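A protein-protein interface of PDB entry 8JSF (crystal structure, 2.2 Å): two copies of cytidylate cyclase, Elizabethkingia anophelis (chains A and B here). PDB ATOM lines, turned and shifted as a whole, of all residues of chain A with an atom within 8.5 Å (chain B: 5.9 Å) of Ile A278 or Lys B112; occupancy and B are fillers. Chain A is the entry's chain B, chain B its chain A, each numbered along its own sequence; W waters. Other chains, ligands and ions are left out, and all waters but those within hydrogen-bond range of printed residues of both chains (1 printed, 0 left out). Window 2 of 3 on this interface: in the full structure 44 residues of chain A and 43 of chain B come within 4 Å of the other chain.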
ATOM      1  N   LEU A 226       3.541 -16.968  13.838  1.00  0.00           N
ATOM      2  CA  LEU A 226       3.428 -18.416  13.757  1.00  0.00           C
ATOM      3  C   LEU A 226       2.127 -18.898  14.383  1.00  0.00           C
ATOM      4  O   LEU A 226       1.502 -19.828  13.870  1.00  0.00           O
ATOM      5  CB  LEU A 226       4.633 -19.072  14.430  1.00  0.00           C
ATOM      6  CG  LEU A 226       4.598 -20.597  14.547  1.00  0.00           C
ATOM      7  CD1 LEU A 226       4.555 -21.232  13.172  1.00  0.00           C
ATOM      8  CD2 LEU A 226       5.800 -21.093  15.333  1.00  0.00           C
ATOM      9  N   LEU A 230      -0.861 -21.166  13.018  1.00  0.00           N
ATOM     10  CA  LEU A 230      -1.081 -22.458  13.651  1.00  0.00           C
ATOM     11  C   LEU A 230      -2.508 -22.594  14.157  1.00  0.00           C
ATOM     12  O   LEU A 230      -3.046 -23.701  14.166  1.00  0.00           O
ATOM     13  CB  LEU A 230      -0.087 -22.675  14.793  1.00  0.00           C
ATOM     14  CG  LEU A 230       1.390 -22.859  14.413  1.00  0.00           C
ATOM     15  CD1 LEU A 230       2.218 -23.219  15.639  1.00  0.00           C
ATOM     16  CD2 LEU A 230       1.569 -23.889  13.307  1.00  0.00           C
ATOM     17  N   LEU A 272       2.018 -37.068  13.102  1.00  0.00           N
ATOM     18  CA  LEU A 272       3.260 -36.487  13.577  1.00  0.00           C
ATOM     19  C   LEU A 272       3.063 -36.011  15.007  1.00  0.00           C
ATOM     20  O   LEU A 272       1.939 -35.706  15.411  1.00  0.00           O
ATOM     21  CB  LEU A 272       3.697 -35.301  12.700  1.00  0.00           C
ATOM     22  CG  LEU A 272       4.280 -35.549  11.303  1.00  0.00           C
ATOM     23  CD1 LEU A 272       3.189 -35.870  10.294  1.00  0.00           C
ATOM     24  CD2 LEU A 272       5.094 -34.341  10.854  1.00  0.00           C
ATOM     25  N   TYR A 274       4.005 -33.207  16.510  1.00  0.00           N
ATOM     26  CA  TYR A 274       3.881 -31.780  16.762  1.00  0.00           C
ATOM     27  C   TYR A 274       3.217 -31.083  15.584  1.00  0.00           C
ATOM     28  O   TYR A 274       3.349 -31.510  14.435  1.00  0.00           O
ATOM     29  CB  TYR A 274       5.259 -31.162  17.032  1.00  0.00           C
ATOM     30  CG  TYR A 274       6.064 -31.943  18.048  1.00  0.00           C
ATOM     31  CD1 TYR A 274       5.739 -31.897  19.396  1.00  0.00           C
ATOM     32  CD2 TYR A 274       7.156 -32.712  17.661  1.00  0.00           C
ATOM     33  CE1 TYR A 274       6.463 -32.609  20.331  1.00  0.00           C
ATOM     34  CE2 TYR A 274       7.895 -33.426  18.593  1.00  0.00           C
ATOM     35  CZ  TYR A 274       7.541 -33.368  19.928  1.00  0.00           C
ATOM     36  OH  TYR A 274       8.254 -34.068  20.878  1.00  0.00           O
ATOM     37  N   VAL A 275       2.502 -29.993  15.885  1.00  0.00           N
ATOM     38  CA  VAL A 275       1.952 -29.153  14.826  1.00  0.00           C
ATOM     39  C   VAL A 275       3.064 -28.405  14.125  1.00  0.00           C
ATOM     40  O   VAL A 275       2.962 -28.093  12.930  1.00  0.00           O
ATOM     41  CB  VAL A 275       0.923 -28.152  15.378  1.00  0.00           C
ATOM     42  CG1 VAL A 275      -0.130 -27.843  14.327  1.00  0.00           C
ATOM     43  CG2 VAL A 275       0.310 -28.673  16.636  1.00  0.00           C
ATOM     44  N   TYR A 276       4.119 -28.071  14.860  1.00  0.00           N
ATOM     45  CA  TYR A 276       5.231 -27.314  14.320  1.00  0.00           C
ATOM     46  C   TYR A 276       6.481 -27.662  15.113  1.00  0.00           C
ATOM     47  O   TYR A 276       6.424 -27.844  16.335  1.00  0.00           O
ATOM     48  CB  TYR A 276       4.959 -25.812  14.386  1.00  0.00           C
ATOM     49  CG  TYR A 276       5.682 -25.022  13.324  1.00  0.00           C
ATOM     50  CD1 TYR A 276       5.217 -25.002  12.016  1.00  0.00           C
ATOM     51  CD2 TYR A 276       6.832 -24.308  13.627  1.00  0.00           C
ATOM     52  CE1 TYR A 276       5.870 -24.277  11.037  1.00  0.00           C
ATOM     53  CE2 TYR A 276       7.498 -23.578  12.653  1.00  0.00           C
ATOM     54  CZ  TYR A 276       7.012 -23.567  11.361  1.00  0.00           C
ATOM     55  OH  TYR A 276       7.663 -22.846  10.390  1.00  0.00           O
ATOM     56  N   GLU A 277       7.602 -27.776  14.410  1.00  0.00           N
ATOM     57  CA  GLU A 277       8.865 -28.109  15.050  1.00  0.00           C
ATOM     58  C   GLU A 277       9.987 -27.299  14.423  1.00  0.00           C
ATOM     59  O   GLU A 277      10.110 -27.251  13.196  1.00  0.00           O
ATOM     60  CB  GLU A 277       9.161 -29.608  14.945  1.00  0.00           C
ATOM     61  CG  GLU A 277       9.903 -30.143  16.151  1.00  0.00           C
ATOM     62  CD  GLU A 277      10.293 -31.596  16.006  1.00  0.00           C
ATOM     63  OE1 GLU A 277       9.911 -32.219  14.990  1.00  0.00           O
ATOM     64  OE2 GLU A 277      10.984 -32.111  16.912  1.00  0.00           O
ATOM     65  N   ILE A 278      10.776 -26.648  15.271  1.00  0.00           N
ATOM     66  CA  ILE A 278      12.041 -26.017  14.901  1.00  0.00           C
ATOM     67  C   ILE A 278      13.122 -26.656  15.765  1.00  0.00           C
ATOM     68  O   ILE A 278      13.325 -26.232  16.913  1.00  0.00           O
ATOM     69  CB  ILE A 278      12.012 -24.493  15.104  1.00  0.00           C
ATOM     70  CG1 ILE A 278      10.786 -23.865  14.445  1.00  0.00           C
ATOM     71  CG2 ILE A 278      13.279 -23.853  14.548  1.00  0.00           C
ATOM     72  CD1 ILE A 278      10.545 -22.433  14.893  1.00  0.00           C
ATOM     73  N   PRO A 279      13.806 -27.695  15.279  1.00  0.00           N
ATOM     74  CA  PRO A 279      14.809 -28.366  16.126  1.00  0.00           C
ATOM     75  C   PRO A 279      15.931 -27.452  16.595  1.00  0.00           C
ATOM     76  O   PRO A 279      16.354 -27.559  17.753  1.00  0.00           O
ATOM     77  CB  PRO A 279      15.329 -29.491  15.219  1.00  0.00           C
ATOM     78  CG  PRO A 279      14.211 -29.743  14.260  1.00  0.00           C
ATOM     79  CD  PRO A 279      13.592 -28.401  14.005  1.00  0.00           C
ATOM     80  N   GLU A 280      16.417 -26.546  15.739  1.00  0.00           N
ATOM     81  CA  GLU A 280      17.511 -25.656  16.124  1.00  0.00           C
ATOM     82  C   GLU A 280      17.170 -24.799  17.336  1.00  0.00           C
ATOM     83  O   GLU A 280      18.081 -24.314  18.013  1.00  0.00           O
ATOM     84  CB  GLU A 280      17.920 -24.756  14.953  1.00  0.00           C
ATOM     85  CG  GLU A 280      18.642 -25.462  13.809  1.00  0.00           C
ATOM     86  CD  GLU A 280      17.811 -26.535  13.136  1.00  0.00           C
ATOM     87  OE1 GLU A 280      16.584 -26.343  12.998  1.00  0.00           O
ATOM     88  OE2 GLU A 280      18.385 -27.577  12.758  1.00  0.00           O
ATOM     89  N   GLU A 281      15.885 -24.597  17.619  1.00  0.00           N
ATOM     90  CA  GLU A 281      15.453 -23.858  18.795  1.00  0.00           C
ATOM     91  C   GLU A 281      14.845 -24.770  19.850  1.00  0.00           C
ATOM     92  O   GLU A 281      14.292 -24.274  20.838  1.00  0.00           O
ATOM     93  CB  GLU A 281      14.443 -22.781  18.402  1.00  0.00           C
ATOM     94  CG  GLU A 281      14.899 -21.878  17.277  1.00  0.00           C
ATOM     95  CD  GLU A 281      13.885 -20.798  16.968  1.00  0.00           C
ATOM     96  OE1 GLU A 281      12.835 -20.758  17.646  1.00  0.00           O
ATOM     97  OE2 GLU A 281      14.131 -19.995  16.045  1.00  0.00           O
ATOM     98  N   TYR A 282      14.936 -26.089  19.661  1.00  0.00           N
ATOM     99  CA  TYR A 282      14.302 -27.059  20.554  1.00  0.00           C
ATOM    100  C   TYR A 282      12.816 -26.744  20.712  1.00  0.00           C
ATOM    101  O   TYR A 282      12.241 -26.864  21.796  1.00  0.00           O
ATOM    102  CB  TYR A 282      15.007 -27.109  21.913  1.00  0.00           C
ATOM    103  CG  TYR A 282      16.509 -27.318  21.835  1.00  0.00           C
ATOM    104  CD1 TYR A 282      17.375 -26.244  21.660  1.00  0.00           C
ATOM    105  CD2 TYR A 282      17.059 -28.590  21.945  1.00  0.00           C
ATOM    106  CE1 TYR A 282      18.745 -26.432  21.590  1.00  0.00           C
ATOM    107  CE2 TYR A 282      18.428 -28.787  21.877  1.00  0.00           C
ATOM    108  CZ  TYR A 282      19.266 -27.705  21.700  1.00  0.00           C
ATOM    109  OH  TYR A 282      20.628 -27.895  21.632  1.00  0.00           O
ATOM    110  N   PHE A 283      12.189 -26.335  19.608  1.00  0.00           N
ATOM    111  CA  PHE A 283      10.800 -25.890  19.604  1.00  0.00           C
ATOM    112  C   PHE A 283       9.932 -27.027  19.081  1.00  0.00           C
ATOM    113  O   PHE A 283      10.010 -27.389  17.906  1.00  0.00           O
ATOM    114  CB  PHE A 283      10.641 -24.632  18.753  1.00  0.00           C
ATOM    115  CG  PHE A 283       9.260 -24.046  18.783  1.00  0.00           C
ATOM    116  CD1 PHE A 283       8.805 -23.367  19.901  1.00  0.00           C
ATOM    117  CD2 PHE A 283       8.425 -24.152  17.683  1.00  0.00           C
ATOM    118  CE1 PHE A 283       7.538 -22.822  19.928  1.00  0.00           C
ATOM    119  CE2 PHE A 283       7.158 -23.606  17.702  1.00  0.00           C
ATOM    120  CZ  PHE A 283       6.715 -22.940  18.827  1.00  0.00           C
ATOM    121  N   ARG A 284       9.106 -27.587  19.959  1.00  0.00           N
ATOM    122  CA  ARG A 284       8.235 -28.715  19.632  1.00  0.00           C
ATOM    123  C   ARG A 284       6.835 -28.363  20.122  1.00  0.00           C
ATOM    124  O   ARG A 284       6.535 -28.520  21.307  1.00  0.00           O
ATOM    125  CB  ARG A 284       8.769 -29.994  20.272  1.00  0.00           C
ATOM    126  CG  ARG A 284      10.197 -30.333  19.833  1.00  0.00           C
ATOM    127  CD  ARG A 284      10.763 -31.574  20.520  1.00  0.00           C
ATOM    128  NE  ARG A 284      10.968 -31.375  21.951  1.00  0.00           N
ATOM    129  CZ  ARG A 284      12.064 -30.850  22.484  1.00  0.00           C
ATOM    130  NH1 ARG A 284      13.082 -30.463  21.732  1.00  0.00           N
ATOM    131  NH2 ARG A 284      12.145 -30.716  23.805  1.00  0.00           N
ATOM    132  N   TYR A 285       5.987 -27.866  19.220  1.00  0.00           N
ATOM    133  CA  TYR A 285       4.696 -27.299  19.590  1.00  0.00           C
ATOM    134  C   TYR A 285       3.609 -28.358  19.459  1.00  0.00           C
ATOM    135  O   TYR A 285       3.380 -28.887  18.366  1.00  0.00           O
ATOM    136  CB  TYR A 285       4.379 -26.082  18.723  1.00  0.00           C
ATOM    137  CG  TYR A 285       3.448 -25.100  19.385  1.00  0.00           C
ATOM    138  CD1 TYR A 285       3.870 -24.347  20.471  1.00  0.00           C
ATOM    139  CD2 TYR A 285       2.153 -24.911  18.914  1.00  0.00           C
ATOM    140  CE1 TYR A 285       3.029 -23.446  21.082  1.00  0.00           C
ATOM    141  CE2 TYR A 285       1.303 -24.007  19.519  1.00  0.00           C
ATOM    142  CZ  TYR A 285       1.747 -23.276  20.601  1.00  0.00           C
ATOM    143  OH  TYR A 285       0.916 -22.370  21.212  1.00  0.00           O
ATOM    144  N   LYS B  22      17.591 -15.456  10.062  1.00  0.00           N
ATOM    145  CA  LYS B  22      17.822 -15.221  11.490  1.00  0.00           C
ATOM    146  C   LYS B  22      19.300 -15.363  11.843  1.00  0.00           C
ATOM    147  O   LYS B  22      19.892 -16.429  11.670  1.00  0.00           O
ATOM    148  CB  LYS B  22      16.984 -16.180  12.346  1.00  0.00           C
ATOM    149  CG  LYS B  22      15.493 -16.149  12.044  1.00  0.00           C
ATOM    150  CD  LYS B  22      14.797 -17.453  12.416  1.00  0.00           C
ATOM    151  CE  LYS B  22      14.328 -17.458  13.860  1.00  0.00           C
ATOM    152  NZ  LYS B  22      13.452 -18.632  14.145  1.00  0.00           N
ATOM    153  N   THR B 108       3.923 -20.871   6.012  1.00  0.00           N
ATOM    154  CA  THR B 108       4.166 -21.058   7.441  1.00  0.00           C
ATOM    155  C   THR B 108       5.540 -21.662   7.704  1.00  0.00           C
ATOM    156  O   THR B 108       6.174 -21.357   8.727  1.00  0.00           O
ATOM    157  CB  THR B 108       3.060 -21.924   8.050  1.00  0.00           C
ATOM    158  OG1 THR B 108       1.785 -21.357   7.726  1.00  0.00           O
ATOM    159  CG2 THR B 108       3.197 -21.990   9.568  1.00  0.00           C
ATOM    160  N   GLY B 109       6.038 -22.490   6.785  1.00  0.00           N
ATOM    161  CA  GLY B 109       7.387 -23.010   6.933  1.00  0.00           C
ATOM    162  C   GLY B 109       8.441 -21.926   6.991  1.00  0.00           C
ATOM    163  O   GLY B 109       9.529 -22.152   7.540  1.00  0.00           O
ATOM    164  N   LEU B 110       8.126 -20.733   6.473  1.00  0.00           N
ATOM    165  CA  LEU B 110       9.072 -19.626   6.541  1.00  0.00           C
ATOM    166  C   LEU B 110       9.475 -19.317   7.972  1.00  0.00           C
ATOM    167  O   LEU B 110      10.584 -18.827   8.207  1.00  0.00           O
ATOM    168  CB  LEU B 110       8.481 -18.377   5.886  1.00  0.00           C
ATOM    169  CG  LEU B 110       8.304 -18.401   4.369  1.00  0.00           C
ATOM    170  CD1 LEU B 110       7.574 -17.146   3.910  1.00  0.00           C
ATOM    171  CD2 LEU B 110       9.651 -18.541   3.668  1.00  0.00           C
ATOM    172  N   PHE B 111       8.608 -19.613   8.944  1.00  0.00           N
ATOM    173  CA  PHE B 111       8.966 -19.279  10.316  1.00  0.00           C
ATOM    174  C   PHE B 111      10.109 -20.128  10.854  1.00  0.00           C
ATOM    175  O   PHE B 111      10.686 -19.768  11.885  1.00  0.00           O
ATOM    176  CB  PHE B 111       7.751 -19.416  11.236  1.00  0.00           C
ATOM    177  CG  PHE B 111       6.715 -18.341  11.042  1.00  0.00           C
ATOM    178  CD1 PHE B 111       6.913 -17.063  11.548  1.00  0.00           C
ATOM    179  CD2 PHE B 111       5.548 -18.607  10.346  1.00  0.00           C
ATOM    180  CE1 PHE B 111       5.960 -16.068  11.365  1.00  0.00           C
ATOM    181  CE2 PHE B 111       4.588 -17.622  10.160  1.00  0.00           C
ATOM    182  CZ  PHE B 111       4.795 -16.350  10.667  1.00  0.00           C
ATOM    183  N   LYS B 112      10.460 -21.235  10.190  1.00  0.00           N
ATOM    184  CA  LYS B 112      11.552 -22.056  10.704  1.00  0.00           C
ATOM    185  C   LYS B 112      12.899 -21.364  10.538  1.00  0.00           C
ATOM    186  O   LYS B 112      13.806 -21.575  11.352  1.00  0.00           O
ATOM    187  CB  LYS B 112      11.559 -23.422  10.020  1.00  0.00           C
ATOM    188  CG  LYS B 112      10.405 -24.316  10.451  1.00  0.00           C
ATOM    189  CD  LYS B 112      10.449 -25.683   9.791  1.00  0.00           C
ATOM    190  CE  LYS B 112       9.253 -26.524  10.218  1.00  0.00           C
ATOM    191  NZ  LYS B 112       9.242 -27.861   9.571  1.00  0.00           N
ATOM    192  N   LYS B 113      13.040 -20.511   9.523  1.00  0.00           N
ATOM    193  CA  LYS B 113      14.306 -19.855   9.242  1.00  0.00           C
ATOM    194  C   LYS B 113      14.248 -18.332   9.252  1.00  0.00           C
ATOM    195  O   LYS B 113      15.306 -17.699   9.153  1.00  0.00           O
ATOM    196  CB  LYS B 113      14.866 -20.323   7.889  1.00  0.00           C
ATOM    197  CG  LYS B 113      15.321 -21.780   7.882  1.00  0.00           C
ATOM    198  CD  LYS B 113      16.682 -21.935   7.213  1.00  0.00           C
ATOM    199  CE  LYS B 113      17.167 -23.375   7.262  1.00  0.00           C
ATOM    200  NZ  LYS B 113      17.312 -23.873   8.658  1.00  0.00           N
ATOM    201  N   PHE B 114      13.069 -17.721   9.360  1.00  0.00           N
ATOM    202  CA  PHE B 114      12.954 -16.276   9.229  1.00  0.00           C
ATOM    203  C   PHE B 114      12.131 -15.690  10.366  1.00  0.00           C
ATOM    204  O   PHE B 114      11.195 -16.314  10.877  1.00  0.00           O
ATOM    205  CB  PHE B 114      12.335 -15.877   7.886  1.00  0.00           C
ATOM    206  CG  PHE B 114      13.171 -16.255   6.701  1.00  0.00           C
ATOM    207  CD1 PHE B 114      14.259 -15.482   6.331  1.00  0.00           C
ATOM    208  CD2 PHE B 114      12.876 -17.386   5.958  1.00  0.00           C
ATOM    209  CE1 PHE B 114      15.032 -15.828   5.240  1.00  0.00           C
ATOM    210  CE2 PHE B 114      13.645 -17.733   4.867  1.00  0.00           C
ATOM    211  CZ  PHE B 114      14.724 -16.955   4.508  1.00  0.00           C
ATOM    212  N   VAL B 191      14.146 -23.613   3.090  1.00  0.00           N
ATOM    213  CA  VAL B 191      12.754 -23.619   3.512  1.00  0.00           C
ATOM    214  C   VAL B 191      11.933 -24.294   2.425  1.00  0.00           C
ATOM    215  O   VAL B 191      12.362 -24.423   1.276  1.00  0.00           O
ATOM    216  CB  VAL B 191      12.211 -22.202   3.800  1.00  0.00           C
ATOM    217  CG1 VAL B 191      12.967 -21.561   4.954  1.00  0.00           C
ATOM    218  CG2 VAL B 191      12.269 -21.337   2.549  1.00  0.00           C
HETATM  219  O   HOH W   1       7.008 -28.386  11.859  1.00  0.00           O
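Leu A226 touches Thr B108 (CD1 to CG2, 3.9 Å). CZ of Phe B111 touches N of Leu A226, at 3.5 Å. Tyr A276 touches Phe B111 (OH to CB, 3.5 Å). O of Glu A277 touches CE of Lys B112, 3.2 Å away. Ile A278 touches Lys B112.
No position is printed for both chains. Of the 9 pairs that touch across the chains among the printed residues, none has its exchanged pair printed and touching as well.
Water W1 lies within hydrogen-bond range of N of Glu A277 and NZ of Lys B112.
Ile A278 touches one residue of chain B. Printed residues of chain A within 4 Å of Lys B112: Tyr A276 (3.1 Å), Glu A277 (3.2 Å) and Ile A278 (3.96 Å). Of the printed residues of chain B, Glu A277 touches Lys B112 (3.2 Å). Printed residues of chain A within 4 Å of Thr B108: Leu A226 and Tyr A276. Of the printed residues of chain A, Gly B109 touches Tyr A276. Of the printed residues of chain B, Glu A281 touches Lys B22. Printed residues of chain B within 4 Å of Tyr A276: Thr B108, Gly B109, Phe B111 and Lys B112. The nearest residue of chain A that does not touch Lys B112 is Glu A281 (5.0 Å). The nearest printed residue of chain B that does not touch Glu A277 is Phe B111 (7.5 Å).
The backbone NH (N) of Tyr A285 lies within hydrogen-bond range of the backbone carbonyl oxygen (O) of Tyr A276. N of Lys B22 sits close to O of Lys B113, at 3.3 Å. The backbone NH (N) of Ile A278 sits at hydrogen-bond distance from the backbone carbonyl oxygen (O) of Phe A283 (2.8 Å).
OH of Tyr A276 lies close to O of Gly B109, at 3.5 Å. The side-chain hydroxyl (OH) of Tyr A276 sits close to the backbone NH (N) of Lys B112, 3.2 Å away. O of Thr B108 is in hydrogen-bond range of OH of Tyr A276 (2.7 Å). The side-chain amino group of Lys B22 lies within salt-bridge range of the side-chain carboxylate of Glu A281, at 2.4 Å.
Of the 9 printed residues of chain B, 5 touch a printed residue of chain A. Hydrophobic or aromatic side chains of chain B within 4 Å of the printed part of chain A: Phe B111. Among the printed residues, Asp or Glu carboxylates within 4 Å of a Lys or Arg side-chain nitrogen of the other chain: Glu A281 with Lys B22 (2.4 Å).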
